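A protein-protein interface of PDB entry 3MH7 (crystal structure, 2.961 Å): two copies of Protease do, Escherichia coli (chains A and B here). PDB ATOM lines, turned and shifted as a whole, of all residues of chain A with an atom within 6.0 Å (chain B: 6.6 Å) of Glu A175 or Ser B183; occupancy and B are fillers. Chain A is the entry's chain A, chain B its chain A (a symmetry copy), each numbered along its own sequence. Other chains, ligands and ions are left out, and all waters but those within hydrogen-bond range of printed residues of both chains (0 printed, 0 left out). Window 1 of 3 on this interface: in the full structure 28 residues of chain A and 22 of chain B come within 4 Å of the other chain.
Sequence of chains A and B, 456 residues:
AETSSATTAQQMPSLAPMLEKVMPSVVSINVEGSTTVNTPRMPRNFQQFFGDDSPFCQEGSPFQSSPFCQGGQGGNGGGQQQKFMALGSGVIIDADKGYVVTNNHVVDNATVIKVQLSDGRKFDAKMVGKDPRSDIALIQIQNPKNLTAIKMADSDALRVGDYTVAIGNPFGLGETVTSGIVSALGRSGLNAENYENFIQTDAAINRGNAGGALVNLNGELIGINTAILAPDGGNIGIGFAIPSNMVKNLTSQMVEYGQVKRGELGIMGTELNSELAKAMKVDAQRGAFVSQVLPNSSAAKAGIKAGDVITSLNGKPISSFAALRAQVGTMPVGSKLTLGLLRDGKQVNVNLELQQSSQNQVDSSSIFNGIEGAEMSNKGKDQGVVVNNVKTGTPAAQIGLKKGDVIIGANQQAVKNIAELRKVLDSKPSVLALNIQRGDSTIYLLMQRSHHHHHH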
ATOM      1  N   VAL A  22     -23.964   0.786   4.319  1.00  0.00           N
ATOM      2  CA  VAL A  22     -25.406   0.914   4.282  1.00  0.00           C
ATOM      3  C   VAL A  22     -25.917   2.345   4.048  1.00  0.00           C
ATOM      4  O   VAL A  22     -26.995   2.549   3.493  1.00  0.00           O
ATOM      5  CB  VAL A  22     -25.993   0.329   5.593  1.00  0.00           C
ATOM      6  CG1 VAL A  22     -27.404   0.792   5.854  1.00  0.00           C
ATOM      7  CG2 VAL A  22     -25.930  -1.165   5.578  1.00  0.00           C
ATOM      8  N   MET A  23     -25.168   3.345   4.491  1.00  0.00           N
ATOM      9  CA  MET A  23     -25.684   4.712   4.449  1.00  0.00           C
ATOM     10  C   MET A  23     -25.983   5.232   3.048  1.00  0.00           C
ATOM     11  O   MET A  23     -26.971   5.933   2.856  1.00  0.00           O
ATOM     12  CB  MET A  23     -24.798   5.669   5.238  1.00  0.00           C
ATOM     13  CG  MET A  23     -25.113   5.628   6.710  1.00  0.00           C
ATOM     14  SD  MET A  23     -23.925   6.657   7.884  1.00  0.00           S
ATOM     15  CE  MET A  23     -22.219   5.793   7.409  1.00  0.00           C
ATOM     16  N   PRO A  24     -25.149   4.873   2.059  1.00  0.00           N
ATOM     17  CA  PRO A  24     -25.424   5.237   0.664  1.00  0.00           C
ATOM     18  C   PRO A  24     -26.848   4.873   0.186  1.00  0.00           C
ATOM     19  O   PRO A  24     -27.442   5.608  -0.579  1.00  0.00           O
ATOM     20  CB  PRO A  24     -24.377   4.431  -0.096  1.00  0.00           C
ATOM     21  CG  PRO A  24     -23.263   4.308   0.860  1.00  0.00           C
ATOM     22  CD  PRO A  24     -23.893   4.113   2.179  1.00  0.00           C
ATOM     23  N   SER A  25     -27.380   3.755   0.654  1.00  0.00           N
ATOM     24  CA  SER A  25     -28.750   3.351   0.404  1.00  0.00           C
ATOM     25  C   SER A  25     -29.836   4.321   0.808  1.00  0.00           C
ATOM     26  O   SER A  25     -30.934   4.266   0.281  1.00  0.00           O
ATOM     27  CB  SER A  25     -29.024   2.084   1.185  1.00  0.00           C
ATOM     28  OG  SER A  25     -29.031   0.983   0.319  1.00  0.00           O
ATOM     29  N   VAL A  26     -29.585   5.165   1.795  1.00  0.00           N
ATOM     30  CA  VAL A  26     -30.666   5.998   2.307  1.00  0.00           C
ATOM     31  C   VAL A  26     -30.498   7.385   1.740  1.00  0.00           C
ATOM     32  O   VAL A  26     -29.366   7.832   1.548  1.00  0.00           O
ATOM     33  CB  VAL A  26     -30.682   6.010   3.841  1.00  0.00           C
ATOM     34  CG1 VAL A  26     -31.858   6.801   4.354  1.00  0.00           C
ATOM     35  CG2 VAL A  26     -30.759   4.590   4.360  1.00  0.00           C
ATOM     36  N   VAL A  27     -31.611   8.045   1.421  1.00  0.00           N
ATOM     37  CA  VAL A  27     -31.544   9.314   0.699  1.00  0.00           C
ATOM     38  C   VAL A  27     -32.433  10.330   1.353  1.00  0.00           C
ATOM     39  O   VAL A  27     -33.334   9.965   2.111  1.00  0.00           O
ATOM     40  CB  VAL A  27     -32.036   9.189  -0.744  1.00  0.00           C
ATOM     41  CG1 VAL A  27     -31.514   7.944  -1.395  1.00  0.00           C
ATOM     42  CG2 VAL A  27     -33.537   9.148  -0.776  1.00  0.00           C
ATOM     43  N   SER A  28     -32.195  11.606   1.049  1.00  0.00           N
ATOM     44  CA  SER A  28     -33.090  12.682   1.489  1.00  0.00           C
ATOM     45  C   SER A  28     -34.036  13.060   0.355  1.00  0.00           C
ATOM     46  O   SER A  28     -33.755  12.839  -0.813  1.00  0.00           O
ATOM     47  CB  SER A  28     -32.308  13.914   1.944  1.00  0.00           C
ATOM     48  OG  SER A  28     -31.055  13.558   2.511  1.00  0.00           O
ATOM     49  N   LEU A 117     -28.462  12.105  -2.509  1.00  0.00           N
ATOM     50  CA  LEU A 117     -27.660  11.040  -1.949  1.00  0.00           C
ATOM     51  C   LEU A 117     -26.842  11.516  -0.760  1.00  0.00           C
ATOM     52  O   LEU A 117     -26.779  12.710  -0.471  1.00  0.00           O
ATOM     53  CB  LEU A 117     -26.725  10.486  -3.010  1.00  0.00           C
ATOM     54  CG  LEU A 117     -27.460   9.970  -4.227  1.00  0.00           C
ATOM     55  CD1 LEU A 117     -26.588   8.977  -4.950  1.00  0.00           C
ATOM     56  CD2 LEU A 117     -28.717   9.324  -3.772  1.00  0.00           C
ATOM     57  N   SER A 118     -26.211  10.570  -0.071  1.00  0.00           N
ATOM     58  CA  SER A 118     -25.392  10.900   1.084  1.00  0.00           C
ATOM     59  C   SER A 118     -24.108  11.581   0.613  1.00  0.00           C
ATOM     60  O   SER A 118     -23.482  12.319   1.368  1.00  0.00           O
ATOM     61  CB  SER A 118     -25.067   9.649   1.896  1.00  0.00           C
ATOM     62  OG  SER A 118     -24.229   8.769   1.167  1.00  0.00           O
ATOM     63  N   ILE A 167     -31.997   5.481  10.220  1.00  0.00           N
ATOM     64  CA  ILE A 167     -31.249   6.414   9.369  1.00  0.00           C
ATOM     65  C   ILE A 167     -32.208   7.301   8.566  1.00  0.00           C
ATOM     66  O   ILE A 167     -33.181   6.809   7.977  1.00  0.00           O
ATOM     67  CB  ILE A 167     -30.376   5.644   8.395  1.00  0.00           C
ATOM     68  CG1 ILE A 167     -29.467   4.704   9.172  1.00  0.00           C
ATOM     69  CG2 ILE A 167     -29.558   6.589   7.524  1.00  0.00           C
ATOM     70  CD1 ILE A 167     -29.329   3.362   8.537  1.00  0.00           C
ATOM     71  N   GLY A 168     -31.954   8.608   8.548  1.00  0.00           N
ATOM     72  CA  GLY A 168     -32.852   9.503   7.853  1.00  0.00           C
ATOM     73  C   GLY A 168     -32.477  10.940   8.047  1.00  0.00           C
ATOM     74  O   GLY A 168     -31.404  11.228   8.553  1.00  0.00           O
ATOM     75  N   ASN A 169     -33.383  11.836   7.665  1.00  0.00           N
ATOM     76  CA  ASN A 169     -33.106  13.263   7.644  1.00  0.00           C
ATOM     77  C   ASN A 169     -33.937  14.127   8.569  1.00  0.00           C
ATOM     78  O   ASN A 169     -34.712  14.957   8.107  1.00  0.00           O
ATOM     79  CB  ASN A 169     -33.315  13.799   6.244  1.00  0.00           C
ATOM     80  CG  ASN A 169     -32.586  15.103   6.019  1.00  0.00           C
ATOM     81  OD1 ASN A 169     -32.077  15.706   6.967  1.00  0.00           O
ATOM     82  ND2 ASN A 169     -32.497  15.530   4.762  1.00  0.00           N
ATOM     83  N   PRO A 170     -33.753  13.985   9.882  1.00  0.00           N
ATOM     84  CA  PRO A 170     -34.525  14.817  10.808  1.00  0.00           C
ATOM     85  C   PRO A 170     -34.282  16.297  10.546  1.00  0.00           C
ATOM     86  O   PRO A 170     -33.120  16.710  10.415  1.00  0.00           O
ATOM     87  CB  PRO A 170     -33.953  14.437  12.179  1.00  0.00           C
ATOM     88  CG  PRO A 170     -32.611  13.904  11.904  1.00  0.00           C
ATOM     89  CD  PRO A 170     -32.691  13.235  10.567  1.00  0.00           C
ATOM     90  N   LEU A 173     -31.363  18.183   8.612  1.00  0.00           N
ATOM     91  CA  LEU A 173     -29.960  18.330   9.013  1.00  0.00           C
ATOM     92  C   LEU A 173     -28.990  17.575   8.099  1.00  0.00           C
ATOM     93  O   LEU A 173     -27.795  17.925   8.010  1.00  0.00           O
ATOM     94  CB  LEU A 173     -29.767  17.827  10.446  1.00  0.00           C
ATOM     95  CG  LEU A 173     -30.237  18.782  11.533  1.00  0.00           C
ATOM     96  CD1 LEU A 173     -30.643  18.038  12.799  1.00  0.00           C
ATOM     97  CD2 LEU A 173     -29.140  19.780  11.790  1.00  0.00           C
ATOM     98  N   GLY A 174     -29.482  16.524   7.446  1.00  0.00           N
ATOM     99  CA  GLY A 174     -28.593  15.643   6.726  1.00  0.00           C
ATOM    100  C   GLY A 174     -28.723  14.252   7.269  1.00  0.00           C
ATOM    101  O   GLY A 174     -29.483  14.048   8.217  1.00  0.00           O
ATOM    102  N   GLU A 175     -27.991  13.306   6.687  1.00  0.00           N
ATOM    103  CA  GLU A 175     -28.159  11.906   7.025  1.00  0.00           C
ATOM    104  C   GLU A 175     -27.729  11.615   8.456  1.00  0.00           C
ATOM    105  O   GLU A 175     -26.532  11.654   8.804  1.00  0.00           O
ATOM    106  CB  GLU A 175     -27.397  11.014   6.065  1.00  0.00           C
ATOM    107  CG  GLU A 175     -27.583   9.530   6.350  1.00  0.00           C
ATOM    108  CD  GLU A 175     -27.080   8.642   5.212  1.00  0.00           C
ATOM    109  OE1 GLU A 175     -26.204   9.099   4.445  1.00  0.00           O
ATOM    110  OE2 GLU A 175     -27.551   7.490   5.085  1.00  0.00           O
ATOM    111  N   THR A 176     -28.726  11.312   9.276  1.00  0.00           N
ATOM    112  CA  THR A 176     -28.534  11.150  10.700  1.00  0.00           C
ATOM    113  C   THR A 176     -28.824   9.706  11.094  1.00  0.00           C
ATOM    114  O   THR A 176     -29.831   9.134  10.665  1.00  0.00           O
ATOM    115  CB  THR A 176     -29.474  12.106  11.438  1.00  0.00           C
ATOM    116  OG1 THR A 176     -29.061  13.445  11.171  1.00  0.00           O
ATOM    117  CG2 THR A 176     -29.452  11.873  12.922  1.00  0.00           C
ATOM    118  N   VAL A 177     -27.935   9.092  11.871  1.00  0.00           N
ATOM    119  CA  VAL A 177     -28.270   7.784  12.411  1.00  0.00           C
ATOM    120  C   VAL A 177     -28.414   7.788  13.923  1.00  0.00           C
ATOM    121  O   VAL A 177     -27.635   8.401  14.663  1.00  0.00           O
ATOM    122  CB  VAL A 177     -27.341   6.667  11.923  1.00  0.00           C
ATOM    123  CG1 VAL A 177     -26.075   7.230  11.359  1.00  0.00           C
ATOM    124  CG2 VAL A 177     -27.025   5.708  13.029  1.00  0.00           C
ATOM    125  N   THR A 178     -29.449   7.096  14.367  1.00  0.00           N
ATOM    126  CA  THR A 178     -29.714   6.957  15.782  1.00  0.00           C
ATOM    127  C   THR A 178     -30.057   5.491  16.006  1.00  0.00           C
ATOM    128  O   THR A 178     -30.394   4.786  15.047  1.00  0.00           O
ATOM    129  CB  THR A 178     -30.868   7.891  16.209  1.00  0.00           C
ATOM    130  OG1 THR A 178     -32.065   7.549  15.507  1.00  0.00           O
ATOM    131  CG2 THR A 178     -30.517   9.325  15.882  1.00  0.00           C
ATOM    132  N   ARG B 159     -15.898   7.942  13.828  1.00  0.00           N
ATOM    133  CA  ARG B 159     -16.783   7.547  12.750  1.00  0.00           C
ATOM    134  C   ARG B 159     -18.220   7.483  13.225  1.00  0.00           C
ATOM    135  O   ARG B 159     -18.504   7.368  14.408  1.00  0.00           O
ATOM    136  CB  ARG B 159     -16.379   6.192  12.206  1.00  0.00           C
ATOM    137  CG  ARG B 159     -15.237   6.221  11.253  1.00  0.00           C
ATOM    138  CD  ARG B 159     -15.028   4.825  10.705  1.00  0.00           C
ATOM    139  NE  ARG B 159     -14.706   3.875  11.770  1.00  0.00           N
ATOM    140  CZ  ARG B 159     -14.692   2.552  11.625  1.00  0.00           C
ATOM    141  NH1 ARG B 159     -15.002   2.005  10.440  1.00  0.00           N
ATOM    142  NH2 ARG B 159     -14.377   1.784  12.676  1.00  0.00           N
ATOM    143  N   VAL B 160     -19.136   7.524  12.282  1.00  0.00           N
ATOM    144  CA  VAL B 160     -20.515   7.683  12.631  1.00  0.00           C
ATOM    145  C   VAL B 160     -21.092   6.475  13.387  1.00  0.00           C
ATOM    146  O   VAL B 160     -21.905   6.636  14.311  1.00  0.00           O
ATOM    147  CB  VAL B 160     -21.311   8.197  11.429  1.00  0.00           C
ATOM    148  CG1 VAL B 160     -22.769   7.876  11.538  1.00  0.00           C
ATOM    149  CG2 VAL B 160     -21.134   9.654  11.384  1.00  0.00           C
ATOM    150  N   ASP B 162     -19.934   5.153  15.875  1.00  0.00           N
ATOM    151  CA  ASP B 162     -19.190   5.027  17.115  1.00  0.00           C
ATOM    152  C   ASP B 162     -19.990   5.255  18.400  1.00  0.00           C
ATOM    153  O   ASP B 162     -20.842   6.134  18.469  1.00  0.00           O
ATOM    154  CB  ASP B 162     -17.963   5.933  17.041  1.00  0.00           C
ATOM    155  CG  ASP B 162     -16.826   5.297  16.224  1.00  0.00           C
ATOM    156  OD1 ASP B 162     -17.024   4.154  15.737  1.00  0.00           O
ATOM    157  OD2 ASP B 162     -15.739   5.921  16.072  1.00  0.00           O
ATOM    158  N   THR B 164     -20.896   6.576  22.087  1.00  0.00           N
ATOM    159  CA  THR B 164     -20.497   7.720  22.887  1.00  0.00           C
ATOM    160  C   THR B 164     -21.184   7.712  24.244  1.00  0.00           C
ATOM    161  O   THR B 164     -22.341   7.310  24.364  1.00  0.00           O
ATOM    162  CB  THR B 164     -20.953   9.000  22.211  1.00  0.00           C
ATOM    163  OG1 THR B 164     -22.389   9.001  22.127  1.00  0.00           O
ATOM    164  CG2 THR B 164     -20.364   9.098  20.818  1.00  0.00           C
ATOM    165  N   ILE B 181     -24.802   7.109  20.271  1.00  0.00           N
ATOM    166  CA  ILE B 181     -23.816   6.940  19.213  1.00  0.00           C
ATOM    167  C   ILE B 181     -23.532   8.254  18.517  1.00  0.00           C
ATOM    168  O   ILE B 181     -24.241   9.242  18.711  1.00  0.00           O
ATOM    169  CB  ILE B 181     -24.289   5.965  18.152  1.00  0.00           C
ATOM    170  CG1 ILE B 181     -25.598   6.451  17.527  1.00  0.00           C
ATOM    171  CG2 ILE B 181     -24.408   4.580  18.733  1.00  0.00           C
ATOM    172  CD1 ILE B 181     -26.066   5.623  16.351  1.00  0.00           C
ATOM    173  N   VAL B 182     -22.489   8.256  17.699  1.00  0.00           N
ATOM    174  CA  VAL B 182     -22.211   9.358  16.801  1.00  0.00           C
ATOM    175  C   VAL B 182     -23.242   9.357  15.673  1.00  0.00           C
ATOM    176  O   VAL B 182     -23.248   8.471  14.842  1.00  0.00           O
ATOM    177  CB  VAL B 182     -20.810   9.194  16.216  1.00  0.00           C
ATOM    178  CG1 VAL B 182     -20.594  10.145  15.050  1.00  0.00           C
ATOM    179  CG2 VAL B 182     -19.753   9.388  17.305  1.00  0.00           C
ATOM    180  N   SER B 183     -24.132  10.335  15.639  1.00  0.00           N
ATOM    181  CA  SER B 183     -25.133  10.330  14.590  1.00  0.00           C
ATOM    182  C   SER B 183     -24.587  10.928  13.300  1.00  0.00           C
ATOM    183  O   SER B 183     -25.075  10.619  12.203  1.00  0.00           O
ATOM    184  CB  SER B 183     -26.367  11.107  15.018  1.00  0.00           C
ATOM    185  OG  SER B 183     -26.917  10.583  16.210  1.00  0.00           O
ATOM    186  N   ALA B 184     -23.580  11.783  13.427  1.00  0.00           N
ATOM    187  CA  ALA B 184     -23.146  12.578  12.294  1.00  0.00           C
ATOM    188  C   ALA B 184     -21.874  13.325  12.642  1.00  0.00           C
ATOM    189  O   ALA B 184     -21.616  13.596  13.816  1.00  0.00           O
ATOM    190  CB  ALA B 184     -24.256  13.564  11.897  1.00  0.00           C
ATOM    191  N   LEU B 185     -21.092  13.678  11.623  1.00  0.00           N
ATOM    192  CA  LEU B 185     -19.893  14.490  11.838  1.00  0.00           C
ATOM    193  C   LEU B 185     -19.920  15.769  11.012  1.00  0.00           C
ATOM    194  O   LEU B 185     -20.551  15.829   9.970  1.00  0.00           O
ATOM    195  CB  LEU B 185     -18.635  13.699  11.515  1.00  0.00           C
ATOM    196  CG  LEU B 185     -18.486  12.411  12.304  1.00  0.00           C
ATOM    197  CD1 LEU B 185     -17.247  11.707  11.900  1.00  0.00           C
ATOM    198  CD2 LEU B 185     -18.469  12.688  13.790  1.00  0.00           C
ATOM    199  N   ARG B 187     -21.253  18.796  11.675  1.00  0.00           N
ATOM    200  CA  ARG B 187     -22.475  19.586  11.573  1.00  0.00           C
ATOM    201  C   ARG B 187     -22.195  21.047  11.889  1.00  0.00           C
ATOM    202  O   ARG B 187     -21.528  21.367  12.866  1.00  0.00           O
ATOM    203  CB  ARG B 187     -23.603  19.027  12.457  1.00  0.00           C
ATOM    204  CG  ARG B 187     -24.140  17.676  12.006  1.00  0.00           C
ATOM    205  CD  ARG B 187     -24.992  17.749  10.732  1.00  0.00           C
ATOM    206  NE  ARG B 187     -25.927  16.622  10.614  1.00  0.00           N
ATOM    207  CZ  ARG B 187     -25.858  15.718   9.650  1.00  0.00           C
ATOM    208  NH1 ARG B 187     -24.918  15.823   8.732  1.00  0.00           N
ATOM    209  NH2 ARG B 187     -26.709  14.717   9.591  1.00  0.00           N
ATOM    210  N   ILE B 199     -19.694  17.331  16.323  1.00  0.00           N
ATOM    211  CA  ILE B 199     -20.118  15.955  16.380  1.00  0.00           C
ATOM    212  C   ILE B 199     -21.582  15.953  16.795  1.00  0.00           C
ATOM    213  O   ILE B 199     -21.987  16.727  17.660  1.00  0.00           O
ATOM    214  CB  ILE B 199     -19.346  15.222  17.450  1.00  0.00           C
ATOM    215  CG1 ILE B 199     -17.888  15.139  17.063  1.00  0.00           C
ATOM    216  CG2 ILE B 199     -19.953  13.830  17.718  1.00  0.00           C
ATOM    217  CD1 ILE B 199     -17.000  14.980  18.252  1.00  0.00           C
ATOM    218  N   GLN B 200     -22.379  15.089  16.178  1.00  0.00           N
ATOM    219  CA  GLN B 200     -23.776  14.967  16.550  1.00  0.00           C
ATOM    220  C   GLN B 200     -24.065  13.619  17.199  1.00  0.00           C
ATOM    221  O   GLN B 200     -23.671  12.564  16.678  1.00  0.00           O
ATOM    222  CB  GLN B 200     -24.657  15.145  15.331  1.00  0.00           C
ATOM    223  CG  GLN B 200     -26.092  15.394  15.695  1.00  0.00           C
ATOM    224  CD  GLN B 200     -27.020  15.320  14.495  1.00  0.00           C
ATOM    225  OE1 GLN B 200     -26.771  15.955  13.460  1.00  0.00           O
ATOM    226  NE2 GLN B 200     -28.098  14.532  14.621  1.00  0.00           N
ATOM    227  N   THR B 201     -24.769  13.645  18.324  1.00  0.00           N
ATOM    228  CA  THR B 201     -25.044  12.413  19.054  1.00  0.00           C
ATOM    229  C   THR B 201     -26.461  12.341  19.611  1.00  0.00           C
ATOM    230  O   THR B 201     -27.110  13.374  19.860  1.00  0.00           O
ATOM    231  CB  THR B 201     -24.080  12.249  20.223  1.00  0.00           C
ATOM    232  OG1 THR B 201     -24.334  10.993  20.861  1.00  0.00           O
ATOM    233  CG2 THR B 201     -24.269  13.399  21.237  1.00  0.00           C
ATOM    234  N   ASP B 202     -26.926  11.112  19.820  1.00  0.00           N
ATOM    235  CA  ASP B 202     -28.234  10.887  20.426  1.00  0.00           C
ATOM    236  C   ASP B 202     -28.155  10.401  21.873  1.00  0.00           C
ATOM    237  O   ASP B 202     -29.146   9.907  22.390  1.00  0.00           O
ATOM    238  CB  ASP B 202     -29.089   9.913  19.603  1.00  0.00           C
ATOM    239  CG  ASP B 202     -28.470   8.508  19.492  1.00  0.00           C
ATOM    240  OD1 ASP B 202     -27.283   8.339  19.842  1.00  0.00           O
ATOM    241  OD2 ASP B 202     -29.174   7.566  19.047  1.00  0.00           O
ATOM    242  N   ALA B 203     -26.983  10.516  22.511  1.00  0.00           N
ATOM    243  CA  ALA B 203     -26.890  10.410  23.967  1.00  0.00           C
ATOM    244  C   ALA B 203     -27.658  11.617  24.487  1.00  0.00           C
ATOM    245  O   ALA B 203     -27.601  12.682  23.861  1.00  0.00           O
ATOM    246  CB  ALA B 203     -25.450  10.455  24.420  1.00  0.00           C
ATOM    247  N   GLY B 237     -33.145  13.663  20.974  1.00  0.00           N
ATOM    248  CA  GLY B 237     -32.302  12.739  20.242  1.00  0.00           C
ATOM    249  C   GLY B 237     -31.251  13.401  19.393  1.00  0.00           C
ATOM    250  O   GLY B 237     -30.481  12.719  18.741  1.00  0.00           O
ATOM    251  N   ILE B 238     -31.203  14.727  19.404  1.00  0.00           N
ATOM    252  CA  ILE B 238     -30.220  15.441  18.609  1.00  0.00           C
ATOM    253  C   ILE B 238     -29.421  16.453  19.428  1.00  0.00           C
ATOM    254  O   ILE B 238     -29.976  17.476  19.835  1.00  0.00           O
ATOM    255  CB  ILE B 238     -30.914  16.232  17.549  1.00  0.00           C
ATOM    256  CG1 ILE B 238     -31.797  15.329  16.705  1.00  0.00           C
ATOM    257  CG2 ILE B 238     -29.902  16.979  16.717  1.00  0.00           C
ATOM    258  CD1 ILE B 238     -32.541  16.089  15.609  1.00  0.00           C
ATOM    259  N   GLY B 239     -28.138  16.171  19.676  1.00  0.00           N
ATOM    260  CA  GLY B 239     -27.280  17.085  20.414  1.00  0.00           C
ATOM    261  C   GLY B 239     -25.908  17.185  19.772  1.00  0.00           C
ATOM    262  O   GLY B 239     -25.537  16.316  18.968  1.00  0.00           O
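NH2 of Arg B187 is in hydrogen-bond range of OG1 of Thr A176 (3.1 Å). The backbone carbonyl oxygen of Leu A173 sits close to the guanidinium group of Arg B187 (3.5 Å). The guanidinium group (NH2) of Arg B187 is in hydrogen-bond range of the backbone carbonyl oxygen (O) of Glu A175, at 3.2 Å. The backbone carbonyl oxygen (O) of Gly A174 sits close to the guanidinium group (NH2) of Arg B187, at 3.2 Å. O of Val A177 lies within hydrogen-bond range of OG of Ser B183 (2.8 Å).
The side-chain amide oxygen of Gln B200 sits at hydrogen-bond distance from the guanidinium group of Arg B187 (3.0 Å). The backbone NH (N) of Leu A173 is in hydrogen-bond range of the side-chain amide oxygen (OD1) of Asn A169, at 3.1 Å. The backbone NH (N) of Ser B183 lies within hydrogen-bond range of the backbone carbonyl oxygen (O) of Gln B200. N of Ile B181 is in hydrogen-bond range of OD1 of Asp B202, at 2.8 Å. O of Gly A174 sits at hydrogen-bond distance from OG1 of Thr A176 (3.0 Å). N of Gly A174 lies within hydrogen-bond range of OD1 of Asn A169 (2.8 Å).
Among the printed residues, pairs that only touch across the chains: Thr A178 with Asp B202 (3.3 Å), Val A177 with Val B160 (3.4 Å), Thr A176 with Gln B200 (3.4 Å), Val A177 with Ile B181 (3.5 Å), Thr A176 with Ser B183 (3.8 Å), Thr A178 with Ser B183 (3.8 Å), Glu A175 with Ser B183 (3.8 Å), Leu A173 with Ile B238 (3.9 Å) and Thr A178 with Ile B181 (3.9 Å).
Of chain B, only Ser B183 and Arg B187 come within 4 Å of Glu A175. Ser B183 touches four residues of chain A. Of the printed residues of chain A, Ile B238 touches Leu A173. Printed residues of chain B within 4 Å of Leu A173: Arg B187 (3.4 Å) and Ile B238 (3.9 Å). Val A22 touches none of the printed residues of chain B.
Of the 19 printed residues of chain A, 6 touch a printed residue of chain B. Hydrophobic or aromatic side chains of chain A within 4 Å of the printed part of chain B: Leu A173 and Val A177. Among the printed residues, no Asp or Glu carboxylate lies within 4 Å of a Lys or Arg side-chain nitrogen of the other chain.
No position is printed for both chains. Of the 14 pairs that touch across the chains among the printed residues, none has its exchanged pair printed and touching as well.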
